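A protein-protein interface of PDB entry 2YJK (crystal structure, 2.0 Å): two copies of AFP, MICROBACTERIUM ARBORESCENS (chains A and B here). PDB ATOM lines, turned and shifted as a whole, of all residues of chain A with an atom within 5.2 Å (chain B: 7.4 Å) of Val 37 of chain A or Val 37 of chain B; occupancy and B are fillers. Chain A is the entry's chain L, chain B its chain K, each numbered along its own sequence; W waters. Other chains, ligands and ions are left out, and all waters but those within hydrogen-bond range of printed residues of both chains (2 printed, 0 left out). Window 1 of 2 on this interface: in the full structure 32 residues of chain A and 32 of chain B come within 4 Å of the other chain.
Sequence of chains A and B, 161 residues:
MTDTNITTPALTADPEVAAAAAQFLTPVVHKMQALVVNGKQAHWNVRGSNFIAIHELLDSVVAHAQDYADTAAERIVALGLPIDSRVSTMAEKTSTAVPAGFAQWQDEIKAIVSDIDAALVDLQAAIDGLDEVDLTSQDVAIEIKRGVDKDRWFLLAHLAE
Val 37 of chain A touches Val 87 of chain B, and with the chains exchanged Val 87 of chain A touches Val 37 of chain B.
Asn 38 of chain A touches Val 87 of chain B, and with the chains exchanged Val 87 of chain A touches Asn 38 of chain B.
Lys 40 of chain A touches Gln 33 of chain B, but with the chains exchanged Gln 33 of chain A does not touch Lys 40 of chain B (4.1 Å).
Positions printed for both chains: 33, 34, 35, 36, 37, 38, 39, 40, 41, 85, 86, 87 and 90.
Of the 24 pairs that touch across the chains among the printed residues, 17 have their exchanged pair printed and touching as well.
Of the 25 printed residues of chain B, 12 touch a printed residue of chain A.
Hydrophobic or aromatic side chains of chain B that line the printed part of chain A: Val 37, Trp 44, Val 87 and Met 90.
Among the printed residues, 24 pairs touch across the chains.
Among the printed residues, no Asp or Glu carboxylate lies within 4 Å of a Lys or Arg side-chain nitrogen of the other chain.
Water W2 lies within hydrogen-bond range of the backbone carbonyl oxygen (O) of Val 98 of chain B (2.7 Å), the guanidinium group (NH1) of Arg 86 of chain A (2.8 Å) and the backbone carbonyl oxygen (O) of Thr 96 of chain B (3.4 Å).
Water W1 lies within hydrogen-bond range of OG of Ser 85 of chain B, O of Val 37 of chain A and NE2 of Gln 33 of chain B.
O of Ala 34 of chain B lies within hydrogen-bond range of ND2 of Asn 38 of chain B (3.4 Å).
The backbone NH (N) of Ala 34 of chain A lies within hydrogen-bond range of the side-chain sulfur (SD) of Met 90 of chain A, at 3.4 Å.
The side-chain amide nitrogen (NE2) of Gln 33 of chain B is in hydrogen-bond range of the side-chain amide oxygen (OE1) of Gln 66 of chain B (3.0 Å).
SD of Met 90 of chain B sits at hydrogen-bond distance from N of Ala 34 of chain B.
ND2 of Asn 38 of chain B sits close to OG1 of Thr 96 of chain B, 3.4 Å away.
N of Ser 85 of chain B lies within hydrogen-bond range of OE1 of Gln 41 of chain A, at 2.9 Å.
OD1 of Asn 38 of chain B is in hydrogen-bond range of N of Val 87 of chain A (3.0 Å).
The side-chain amide oxygen (OE1) of Gln 41 of chain B sits at hydrogen-bond distance from the backbone NH (N) of Ser 85 of chain A.
The side-chain amide oxygen (OD1) of Asn 38 of chain A is in hydrogen-bond range of the backbone NH (N) of Val 87 of chain B (2.9 Å).
Among the printed residues, pairs that only touch across the chains: Arg 86 of chain A with Val 98 of chain B (3.2 Å), Ser 85 of chain A with Val 37 of chain B (3.3 Å), Val 37 of chain A with Ser 85 of chain B (3.3 Å), Asn 38 of chain A with Arg 86 of chain B (3.4 Å), Arg 86 of chain A with Asn 38 of chain B (3.5 Å), Val 87 of chain A with Val 37 of chain B (3.5 Å), Val 37 of chain A with Val 87 of chain B (3.5 Å), Gln 33 of chain A with Trp 44 of chain B (3.6 Å), Met 90 of chain A with Val 87 of chain B (3.6 Å), Lys 40 of chain A with Gln 66 of chain B (3.7 Å), Val 87 of chain A with Met 90 of chain B (3.7 Å), Ser 85 of chain A with Trp 44 of chain B (3.7 Å), Gln 41 of chain A with Arg 86 of chain B (3.8 Å), Val 87 of chain A with Ala 34 of chain B (3.8 Å), Arg 86 of chain A with Gln 41 of chain B (3.8 Å), Gln 33 of chain A with Val 37 of chain B (3.9 Å), Val 36 of chain A with Gln 66 of chain B (3.9 Å), Lys 40 of chain A with Gln 33 of chain B (3.95 Å), Ala 34 of chain A with Val 87 of chain B (3.96 Å) and Val 37 of chain A with Val 37 of chain B (3.99 Å).
Of the printed residues of chain B, Val 37 of chain A touches Val 37, Ser 85 and Val 87.
Printed residues of chain B within 4 Å of Val 87 of chain A: Ala 34, Val 37, Asn 38 and Met 90.
Printed residues of chain A within 4 Å of Val 37 of chain B: Gln 33, Val 37, Ser 85 and Val 87.
Ser 88 of chain B touches none of the printed residues of chain A.
Of the printed residues of chain A, Met 90 of chain B touches Val 87.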
ATOM      1  N   GLN A  33      24.484  -4.628  12.073  1.00  0.00           N
ATOM      2  CA  GLN A  33      24.809  -4.425  13.459  1.00  0.00           C
ATOM      3  C   GLN A  33      25.556  -3.091  13.665  1.00  0.00           C
ATOM      4  O   GLN A  33      25.359  -2.446  14.710  1.00  0.00           O
ATOM      5  CB  GLN A  33      25.600  -5.630  14.016  1.00  0.00           C
ATOM      6  CG  GLN A  33      25.807  -5.620  15.585  1.00  0.00           C
ATOM      7  CD  GLN A  33      24.468  -5.553  16.350  1.00  0.00           C
ATOM      8  OE1 GLN A  33      24.080  -4.485  16.902  1.00  0.00           O
ATOM      9  NE2 GLN A  33      23.734  -6.621  16.319  1.00  0.00           N
ATOM     10  N   ALA A  34      26.437  -2.715  12.726  1.00  0.00           N
ATOM     11  CA  ALA A  34      27.108  -1.400  12.706  1.00  0.00           C
ATOM     12  C   ALA A  34      26.071  -0.279  12.537  1.00  0.00           C
ATOM     13  O   ALA A  34      26.186   0.778  13.139  1.00  0.00           O
ATOM     14  CB  ALA A  34      28.215  -1.310  11.524  1.00  0.00           C
ATOM     15  N   LEU A  35      25.048  -0.500  11.713  1.00  0.00           N
ATOM     16  CA  LEU A  35      24.023   0.524  11.502  1.00  0.00           C
ATOM     17  C   LEU A  35      23.222   0.763  12.794  1.00  0.00           C
ATOM     18  O   LEU A  35      22.839   1.885  13.064  1.00  0.00           O
ATOM     19  CB  LEU A  35      23.108   0.170  10.311  1.00  0.00           C
ATOM     20  CG  LEU A  35      22.041   1.208   9.941  1.00  0.00           C
ATOM     21  CD1 LEU A  35      22.726   2.482   9.326  1.00  0.00           C
ATOM     22  CD2 LEU A  35      21.012   0.658   8.916  1.00  0.00           C
ATOM     23  N   VAL A  36      23.025  -0.273  13.619  1.00  0.00           N
ATOM     24  CA  VAL A  36      22.478  -0.065  14.980  1.00  0.00           C
ATOM     25  C   VAL A  36      23.346   0.980  15.804  1.00  0.00           C
ATOM     26  O   VAL A  36      22.796   1.941  16.395  1.00  0.00           O
ATOM     27  CB  VAL A  36      22.394  -1.388  15.774  1.00  0.00           C
ATOM     28  CG1 VAL A  36      22.076  -1.181  17.289  1.00  0.00           C
ATOM     29  CG2 VAL A  36      21.360  -2.359  15.122  1.00  0.00           C
ATOM     30  N   VAL A  37      24.656   0.758  15.864  1.00  0.00           N
ATOM     31  CA  VAL A  37      25.535   1.576  16.679  1.00  0.00           C
ATOM     32  C   VAL A  37      25.711   2.984  16.074  1.00  0.00           C
ATOM     33  O   VAL A  37      25.547   3.978  16.770  1.00  0.00           O
ATOM     34  CB  VAL A  37      26.928   0.947  16.771  1.00  0.00           C
ATOM     35  CG1 VAL A  37      27.928   1.899  17.452  1.00  0.00           C
ATOM     36  CG2 VAL A  37      26.806  -0.378  17.452  1.00  0.00           C
ATOM     37  N   ASN A  38      25.999   3.049  14.773  1.00  0.00           N
ATOM     38  CA  ASN A  38      26.214   4.330  14.101  1.00  0.00           C
ATOM     39  C   ASN A  38      24.879   5.119  13.933  1.00  0.00           C
ATOM     40  O   ASN A  38      24.873   6.371  13.913  1.00  0.00           O
ATOM     41  CB  ASN A  38      26.952   4.079  12.761  1.00  0.00           C
ATOM     42  CG  ASN A  38      28.344   3.509  12.980  1.00  0.00           C
ATOM     43  OD1 ASN A  38      29.071   3.953  13.895  1.00  0.00           O
ATOM     44  ND2 ASN A  38      28.766   2.574  12.118  1.00  0.00           N
ATOM     45  N   GLY A  39      23.770   4.392  13.796  1.00  0.00           N
ATOM     46  CA  GLY A  39      22.405   5.024  13.783  1.00  0.00           C
ATOM     47  C   GLY A  39      22.084   5.690  15.118  1.00  0.00           C
ATOM     48  O   GLY A  39      21.476   6.778  15.163  1.00  0.00           O
ATOM     49  N   LYS A  40      22.469   5.035  16.220  1.00  0.00           N
ATOM     50  CA  LYS A  40      22.240   5.576  17.598  1.00  0.00           C
ATOM     51  C   LYS A  40      23.134   6.812  17.729  1.00  0.00           C
ATOM     52  O   LYS A  40      22.756   7.870  18.305  1.00  0.00           O
ATOM     53  CB  LYS A  40      22.683   4.545  18.661  1.00  0.00           C
ATOM     54  CG  LYS A  40      21.602   3.534  19.131  1.00  0.00           C
ATOM     55  CD  LYS A  40      20.394   4.329  19.660  1.00  0.00           C
ATOM     56  CE  LYS A  40      19.326   3.345  20.210  1.00  0.00           C
ATOM     57  NZ  LYS A  40      18.075   4.042  20.743  1.00  0.00           N
ATOM     58  N   GLN A  41      24.333   6.693  17.176  1.00  0.00           N
ATOM     59  CA  GLN A  41      25.240   7.830  17.223  1.00  0.00           C
ATOM     60  C   GLN A  41      24.532   9.027  16.541  1.00  0.00           C
ATOM     61  O   GLN A  41      24.480  10.111  17.085  1.00  0.00           O
ATOM     62  CB  GLN A  41      26.590   7.464  16.555  1.00  0.00           C
ATOM     63  CG  GLN A  41      27.480   8.656  16.185  1.00  0.00           C
ATOM     64  CD  GLN A  41      28.131   9.264  17.420  1.00  0.00           C
ATOM     65  OE1 GLN A  41      27.983   8.734  18.535  1.00  0.00           O
ATOM     66  NE2 GLN A  41      28.892  10.356  17.233  1.00  0.00           N
ATOM     67  N   SER A  85      30.341 -11.798  15.264  1.00  0.00           N
ATOM     68  CA  SER A  85      30.008 -10.390  15.256  1.00  0.00           C
ATOM     69  C   SER A  85      30.483  -9.668  16.550  1.00  0.00           C
ATOM     70  O   SER A  85      29.798  -8.760  17.035  1.00  0.00           O
ATOM     71  CB  SER A  85      28.483 -10.205  15.089  1.00  0.00           C
ATOM     72  OG  SER A  85      28.211  -8.869  14.684  1.00  0.00           O
ATOM     73  N   ARG A  86      31.609 -10.062  17.140  1.00  0.00           N
ATOM     74  CA  ARG A  86      32.168  -9.292  18.262  1.00  0.00           C
ATOM     75  C   ARG A  86      32.433  -7.848  17.775  1.00  0.00           C
ATOM     76  O   ARG A  86      32.615  -7.570  16.563  1.00  0.00           O
ATOM     77  CB  ARG A  86      33.432  -9.928  18.732  1.00  0.00           C
ATOM     78  CG  ARG A  86      33.280 -11.320  19.258  1.00  0.00           C
ATOM     79  CD  ARG A  86      34.678 -11.902  19.651  1.00  0.00           C
ATOM     80  NE  ARG A  86      35.373 -12.172  18.415  1.00  0.00           N
ATOM     81  CZ  ARG A  86      36.661 -12.451  18.282  1.00  0.00           C
ATOM     82  NH1 ARG A  86      37.455 -12.581  19.320  1.00  0.00           N
ATOM     83  NH2 ARG A  86      37.128 -12.630  17.060  1.00  0.00           N
ATOM     84  N   VAL A  87      32.447  -6.907  18.696  1.00  0.00           N
ATOM     85  CA  VAL A  87      32.718  -5.505  18.329  1.00  0.00           C
ATOM     86  C   VAL A  87      34.024  -5.348  17.510  1.00  0.00           C
ATOM     87  O   VAL A  87      34.088  -4.582  16.526  1.00  0.00           O
ATOM     88  CB  VAL A  87      32.758  -4.604  19.625  1.00  0.00           C
ATOM     89  CG1 VAL A  87      33.374  -3.196  19.345  1.00  0.00           C
ATOM     90  CG2 VAL A  87      31.309  -4.482  20.249  1.00  0.00           C
ATOM     91  N   MET A  90      33.465  -6.619  14.004  1.00  0.00           N
ATOM     92  CA  MET A  90      32.549  -5.721  13.321  1.00  0.00           C
ATOM     93  C   MET A  90      33.251  -4.408  12.944  1.00  0.00           C
ATOM     94  O   MET A  90      33.067  -3.911  11.834  1.00  0.00           O
ATOM     95  CB  MET A  90      31.292  -5.475  14.158  1.00  0.00           C
ATOM     96  CG  MET A  90      30.326  -4.457  13.544  1.00  0.00           C
ATOM     97  SD  MET A  90      28.958  -4.001  14.699  1.00  0.00           S
ATOM     98  CE  MET A  90      29.869  -3.073  15.949  1.00  0.00           C
ATOM     99  N   LYS B  31      30.826   1.131  27.035  1.00  0.00           N
ATOM    100  CA  LYS B  31      30.752  -0.260  27.477  1.00  0.00           C
ATOM    101  C   LYS B  31      29.347  -0.799  27.395  1.00  0.00           C
ATOM    102  O   LYS B  31      29.177  -1.952  27.138  1.00  0.00           O
ATOM    103  CB  LYS B  31      31.248  -0.347  28.881  1.00  0.00           C
ATOM    104  CG  LYS B  31      32.751  -0.026  28.946  1.00  0.00           C
ATOM    105  CD  LYS B  31      33.287  -0.420  30.313  1.00  0.00           C
ATOM    106  CE  LYS B  31      34.855  -0.608  30.312  1.00  0.00           C
ATOM    107  NZ  LYS B  31      35.475   0.719  30.250  1.00  0.00           N
ATOM    108  N   MET B  32      28.323   0.021  27.641  1.00  0.00           N
ATOM    109  CA  MET B  32      26.924  -0.467  27.468  1.00  0.00           C
ATOM    110  C   MET B  32      26.561  -0.752  26.029  1.00  0.00           C
ATOM    111  O   MET B  32      25.886  -1.774  25.752  1.00  0.00           O
ATOM    112  CB  MET B  32      25.843   0.435  28.116  1.00  0.00           C
ATOM    113  CG  MET B  32      25.938   0.539  29.594  1.00  0.00           C
ATOM    114  SD  MET B  32      25.634  -1.050  30.416  1.00  0.00           S
ATOM    115  CE  MET B  32      27.199  -1.271  31.170  1.00  0.00           C
ATOM    116  N   GLN B  33      26.983   0.136  25.112  1.00  0.00           N
ATOM    117  CA  GLN B  33      26.780  -0.080  23.669  1.00  0.00           C
ATOM    118  C   GLN B  33      27.606  -1.273  23.147  1.00  0.00           C
ATOM    119  O   GLN B  33      27.165  -1.993  22.231  1.00  0.00           O
ATOM    120  CB  GLN B  33      27.044   1.203  22.876  1.00  0.00           C
ATOM    121  CG  GLN B  33      26.641   1.111  21.427  1.00  0.00           C
ATOM    122  CD  GLN B  33      25.134   0.969  21.273  1.00  0.00           C
ATOM    123  OE1 GLN B  33      24.598  -0.134  20.979  1.00  0.00           O
ATOM    124  NE2 GLN B  33      24.437   2.062  21.456  1.00  0.00           N
ATOM    125  N   ALA B  34      28.786  -1.499  23.723  1.00  0.00           N
ATOM    126  CA  ALA B  34      29.599  -2.707  23.399  1.00  0.00           C
ATOM    127  C   ALA B  34      28.915  -4.011  23.869  1.00  0.00           C
ATOM    128  O   ALA B  34      28.859  -4.993  23.119  1.00  0.00           O
ATOM    129  CB  ALA B  34      31.063  -2.623  23.969  1.00  0.00           C
ATOM    130  N   LEU B  35      28.419  -3.996  25.105  1.00  0.00           N
ATOM    131  CA  LEU B  35      27.597  -5.040  25.643  1.00  0.00           C
ATOM    132  C   LEU B  35      26.340  -5.420  24.790  1.00  0.00           C
ATOM    133  O   LEU B  35      25.989  -6.605  24.717  1.00  0.00           O
ATOM    134  CB  LEU B  35      27.197  -4.691  27.073  1.00  0.00           C
ATOM    135  CG  LEU B  35      26.362  -5.746  27.851  1.00  0.00           C
ATOM    136  CD1 LEU B  35      27.043  -7.104  27.827  1.00  0.00           C
ATOM    137  CD2 LEU B  35      26.072  -5.324  29.372  1.00  0.00           C
ATOM    138  N   VAL B  36      25.695  -4.450  24.127  1.00  0.00           N
ATOM    139  CA  VAL B  36      24.642  -4.747  23.170  1.00  0.00           C
ATOM    140  C   VAL B  36      25.217  -5.673  22.113  1.00  0.00           C
ATOM    141  O   VAL B  36      24.601  -6.685  21.806  1.00  0.00           O
ATOM    142  CB  VAL B  36      24.023  -3.479  22.496  1.00  0.00           C
ATOM    143  CG1 VAL B  36      22.985  -3.840  21.378  1.00  0.00           C
ATOM    144  CG2 VAL B  36      23.332  -2.606  23.589  1.00  0.00           C
ATOM    145  N   VAL B  37      26.389  -5.320  21.559  1.00  0.00           N
ATOM    146  CA  VAL B  37      26.887  -6.055  20.396  1.00  0.00           C
ATOM    147  C   VAL B  37      27.475  -7.400  20.797  1.00  0.00           C
ATOM    148  O   VAL B  37      27.149  -8.438  20.184  1.00  0.00           O
ATOM    149  CB  VAL B  37      27.946  -5.236  19.660  1.00  0.00           C
ATOM    150  CG1 VAL B  37      28.683  -6.099  18.586  1.00  0.00           C
ATOM    151  CG2 VAL B  37      27.293  -4.022  19.001  1.00  0.00           C
ATOM    152  N   ASN B  38      28.307  -7.390  21.846  1.00  0.00           N
ATOM    153  CA  ASN B  38      28.904  -8.645  22.321  1.00  0.00           C
ATOM    154  C   ASN B  38      27.890  -9.543  22.995  1.00  0.00           C
ATOM    155  O   ASN B  38      28.057 -10.749  22.984  1.00  0.00           O
ATOM    156  CB  ASN B  38      30.151  -8.421  23.195  1.00  0.00           C
ATOM    157  CG  ASN B  38      31.178  -7.616  22.482  1.00  0.00           C
ATOM    158  OD1 ASN B  38      31.431  -7.871  21.326  1.00  0.00           O
ATOM    159  ND2 ASN B  38      31.797  -6.621  23.167  1.00  0.00           N
ATOM    160  N   GLY B  39      26.817  -8.963  23.516  1.00  0.00           N
ATOM    161  CA  GLY B  39      25.694  -9.759  24.072  1.00  0.00           C
ATOM    162  C   GLY B  39      24.916 -10.452  22.959  1.00  0.00           C
ATOM    163  O   GLY B  39      24.498 -11.612  23.115  1.00  0.00           O
ATOM    164  N   LYS B  40      24.695  -9.760  21.839  1.00  0.00           N
ATOM    165  CA  LYS B  40      24.012 -10.420  20.683  1.00  0.00           C
ATOM    166  C   LYS B  40      24.874 -11.544  20.200  1.00  0.00           C
ATOM    167  O   LYS B  40      24.420 -12.629  19.949  1.00  0.00           O
ATOM    168  CB  LYS B  40      23.730  -9.429  19.496  1.00  0.00           C
ATOM    169  CG  LYS B  40      22.433  -8.631  19.706  1.00  0.00           C
ATOM    170  CD  LYS B  40      21.190  -9.542  19.824  1.00  0.00           C
ATOM    171  CE  LYS B  40      19.900  -8.702  19.707  1.00  0.00           C
ATOM    172  NZ  LYS B  40      18.772  -9.632  19.523  1.00  0.00           N
ATOM    173  N   GLN B  41      26.152 -11.288  20.073  1.00  0.00           N
ATOM    174  CA  GLN B  41      27.102 -12.370  19.710  1.00  0.00           C
ATOM    175  C   GLN B  41      26.939 -13.623  20.589  1.00  0.00           C
ATOM    176  O   GLN B  41      26.809 -14.761  20.064  1.00  0.00           O
ATOM    177  CB  GLN B  41      28.559 -11.844  19.854  1.00  0.00           C
ATOM    178  CG  GLN B  41      29.698 -12.948  19.753  1.00  0.00           C
ATOM    179  CD  GLN B  41      29.900 -13.437  18.317  1.00  0.00           C
ATOM    180  OE1 GLN B  41      29.179 -12.986  17.408  1.00  0.00           O
ATOM    181  NE2 GLN B  41      30.839 -14.379  18.106  1.00  0.00           N
ATOM    182  N   ALA B  42      26.993 -13.429  21.927  1.00  0.00           N
ATOM    183  CA  ALA B  42      26.831 -14.507  22.899  1.00  0.00           C
ATOM    184  C   ALA B  42      25.431 -15.180  22.737  1.00  0.00           C
ATOM    185  O   ALA B  42      25.310 -16.364  22.815  1.00  0.00           O
ATOM    186  CB  ALA B  42      27.024 -13.962  24.318  1.00  0.00           C
ATOM    187  N   HIS B  43      24.407 -14.391  22.447  1.00  0.00           N
ATOM    188  CA  HIS B  43      23.035 -14.884  22.267  1.00  0.00           C
ATOM    189  C   HIS B  43      22.886 -15.780  21.026  1.00  0.00           C
ATOM    190  O   HIS B  43      22.116 -16.766  21.043  1.00  0.00           O
ATOM    191  CB  HIS B  43      22.151 -13.600  22.164  1.00  0.00           C
ATOM    192  CG  HIS B  43      20.796 -13.770  21.589  1.00  0.00           C
ATOM    193  ND1 HIS B  43      19.730 -14.249  22.332  1.00  0.00           N
ATOM    194  CD2 HIS B  43      20.281 -13.388  20.403  1.00  0.00           C
ATOM    195  CE1 HIS B  43      18.637 -14.210  21.605  1.00  0.00           C
ATOM    196  NE2 HIS B  43      18.935 -13.663  20.443  1.00  0.00           N
ATOM    197  N   TRP B  44      23.566 -15.418  19.947  1.00  0.00           N
ATOM    198  CA  TRP B  44      23.466 -16.187  18.700  1.00  0.00           C
ATOM    199  C   TRP B  44      24.244 -17.470  18.777  1.00  0.00           C
ATOM    200  O   TRP B  44      23.793 -18.512  18.240  1.00  0.00           O
ATOM    201  CB  TRP B  44      24.030 -15.379  17.543  1.00  0.00           C
ATOM    202  CG  TRP B  44      23.139 -14.157  17.207  1.00  0.00           C
ATOM    203  CD1 TRP B  44      21.757 -14.072  17.301  1.00  0.00           C
ATOM    204  CD2 TRP B  44      23.600 -12.887  16.797  1.00  0.00           C
ATOM    205  NE1 TRP B  44      21.351 -12.811  16.926  1.00  0.00           N
ATOM    206  CE2 TRP B  44      22.448 -12.070  16.579  1.00  0.00           C
ATOM    207  CE3 TRP B  44      24.871 -12.382  16.469  1.00  0.00           C
ATOM    208  CZ2 TRP B  44      22.528 -10.741  16.086  1.00  0.00           C
ATOM    209  CZ3 TRP B  44      24.962 -11.018  15.982  1.00  0.00           C
ATOM    210  CH2 TRP B  44      23.805 -10.231  15.830  1.00  0.00           C
ATOM    211  N   VAL B  62      20.792  -7.579  26.786  1.00  0.00           N
ATOM    212  CA  VAL B  62      21.125  -6.765  25.631  1.00  0.00           C
ATOM    213  C   VAL B  62      20.117  -5.581  25.511  1.00  0.00           C
ATOM    214  O   VAL B  62      20.515  -4.444  25.301  1.00  0.00           O
ATOM    215  CB  VAL B  62      21.161  -7.619  24.334  1.00  0.00           C
ATOM    216  CG1 VAL B  62      20.883  -6.792  23.106  1.00  0.00           C
ATOM    217  CG2 VAL B  62      22.466  -8.387  24.238  1.00  0.00           C
ATOM    218  N   ALA B  65      21.026  -3.199  28.298  1.00  0.00           N
ATOM    219  CA  ALA B  65      22.249  -2.481  27.973  1.00  0.00           C
ATOM    220  C   ALA B  65      21.964  -1.372  26.930  1.00  0.00           C
ATOM    221  O   ALA B  65      22.578  -0.316  26.998  1.00  0.00           O
ATOM    222  CB  ALA B  65      23.353  -3.441  27.428  1.00  0.00           C
ATOM    223  N   GLN B  66      21.096  -1.660  25.953  1.00  0.00           N
ATOM    224  CA  GLN B  66      20.718  -0.656  24.940  1.00  0.00           C
ATOM    225  C   GLN B  66      20.029   0.573  25.595  1.00  0.00           C
ATOM    226  O   GLN B  66      20.309   1.742  25.201  1.00  0.00           O
ATOM    227  CB  GLN B  66      19.810  -1.202  23.788  1.00  0.00           C
ATOM    228  CG  GLN B  66      19.656  -0.179  22.615  1.00  0.00           C
ATOM    229  CD  GLN B  66      21.091   0.269  21.970  1.00  0.00           C
ATOM    230  OE1 GLN B  66      21.675   1.352  22.265  1.00  0.00           O
ATOM    231  NE2 GLN B  66      21.621  -0.587  21.129  1.00  0.00           N
ATOM    232  N   SER B  85      30.232   7.746  20.025  1.00  0.00           N
ATOM    233  CA  SER B  85      30.255   6.293  20.074  1.00  0.00           C
ATOM    234  C   SER B  85      30.006   5.649  18.696  1.00  0.00           C
ATOM    235  O   SER B  85      29.146   4.751  18.560  1.00  0.00           O
ATOM    236  CB  SER B  85      29.296   5.740  21.125  1.00  0.00           C
ATOM    237  OG  SER B  85      27.994   5.783  20.634  1.00  0.00           O
ATOM    238  N   ARG B  86      30.656   6.182  17.673  1.00  0.00           N
ATOM    239  CA  ARG B  86      30.737   5.456  16.385  1.00  0.00           C
ATOM    240  C   ARG B  86      31.396   4.074  16.648  1.00  0.00           C
ATOM    241  O   ARG B  86      32.132   3.871  17.661  1.00  0.00           O
ATOM    242  CB  ARG B  86      31.574   6.201  15.375  1.00  0.00           C
ATOM    243  CG  ARG B  86      31.050   7.514  14.923  1.00  0.00           C
ATOM    244  CD  ARG B  86      32.144   8.228  14.127  1.00  0.00           C
ATOM    245  NE  ARG B  86      33.269   8.719  14.930  1.00  0.00           N
ATOM    246  CZ  ARG B  86      34.421   9.196  14.445  1.00  0.00           C
ATOM    247  NH1 ARG B  86      34.645   9.257  13.145  1.00  0.00           N
ATOM    248  NH2 ARG B  86      35.344   9.650  15.275  1.00  0.00           N
ATOM    249  N   VAL B  87      31.183   3.134  15.720  1.00  0.00           N
ATOM    250  CA  VAL B  87      31.743   1.805  15.920  1.00  0.00           C
ATOM    251  C   VAL B  87      33.265   1.865  16.189  1.00  0.00           C
ATOM    252  O   VAL B  87      33.808   1.156  17.039  1.00  0.00           O
ATOM    253  CB  VAL B  87      31.383   0.872  14.780  1.00  0.00           C
ATOM    254  CG1 VAL B  87      32.261  -0.326  14.774  1.00  0.00           C
ATOM    255  CG2 VAL B  87      29.859   0.420  14.901  1.00  0.00           C
ATOM    256  N   SER B  88      33.951   2.692  15.423  1.00  0.00           N
ATOM    257  CA  SER B  88      35.412   2.725  15.458  1.00  0.00           C
ATOM    258  C   SER B  88      35.918   3.214  16.824  1.00  0.00           C
ATOM    259  O   SER B  88      36.911   2.722  17.299  1.00  0.00           O
ATOM    260  CB  SER B  88      35.959   3.612  14.297  1.00  0.00           C
ATOM    261  OG  SER B  88      35.493   4.959  14.408  1.00  0.00           O
ATOM    262  N   MET B  90      34.057   3.213  19.679  1.00  0.00           N
ATOM    263  CA  MET B  90      33.642   2.192  20.633  1.00  0.00           C
ATOM    264  C   MET B  90      34.617   1.001  20.613  1.00  0.00           C
ATOM    265  O   MET B  90      34.996   0.527  21.697  1.00  0.00           O
ATOM    266  CB  MET B  90      32.194   1.755  20.409  1.00  0.00           C
ATOM    267  CG  MET B  90      31.687   0.702  21.325  1.00  0.00           C
ATOM    268  SD  MET B  90      30.086   0.022  20.720  1.00  0.00           S
ATOM    269  CE  MET B  90      30.525  -0.824  19.212  1.00  0.00           C
ATOM    270  N   THR B  96      36.423  -7.372  24.693  1.00  0.00           N
ATOM    271  CA  THR B  96      35.459  -8.383  25.080  1.00  0.00           C
ATOM    272  C   THR B  96      36.121  -9.741  25.331  1.00  0.00           C
ATOM    273  O   THR B  96      37.016 -10.118  24.611  1.00  0.00           O
ATOM    274  CB  THR B  96      34.355  -8.523  24.007  1.00  0.00           C
ATOM    275  OG1 THR B  96      33.349  -9.400  24.479  1.00  0.00           O
ATOM    276  CG2 THR B  96      34.908  -9.064  22.680  1.00  0.00           C
ATOM    277  N   VAL B  98      33.936 -12.388  25.074  1.00  0.00           N
ATOM    278  CA  VAL B  98      32.996 -13.267  24.344  1.00  0.00           C
ATOM    279  C   VAL B  98      33.755 -13.955  23.254  1.00  0.00           C
ATOM    280  O   VAL B  98      34.432 -13.278  22.512  1.00  0.00           O
ATOM    281  CB  VAL B  98      31.748 -12.478  23.788  1.00  0.00           C
ATOM    282  CG1 VAL B  98      30.796 -13.385  22.978  1.00  0.00           C
ATOM    283  CG2 VAL B  98      30.985 -11.804  24.962  1.00  0.00           C
ATOM    284  N   ILE B 112      30.414 -12.700  29.509  1.00  0.00           N
ATOM    285  CA  ILE B 112      29.530 -11.570  29.730  1.00  0.00           C
ATOM    286  C   ILE B 112      29.676 -10.926  31.140  1.00  0.00           C
ATOM    287  O   ILE B 112      29.612  -9.690  31.293  1.00  0.00           O
ATOM    288  CB  ILE B 112      28.015 -11.958  29.442  1.00  0.00           C
ATOM    289  CG1 ILE B 112      27.795 -12.276  27.934  1.00  0.00           C
ATOM    290  CG2 ILE B 112      27.102 -10.818  29.838  1.00  0.00           C
ATOM    291  CD1 ILE B 112      28.038 -11.053  27.031  1.00  0.00           C
HETATM  292  O   HOH W   1      26.306   4.016  19.508  1.00  0.00           O
HETATM  293  O   HOH W   2      36.882 -12.358  22.023  1.00  0.00           O
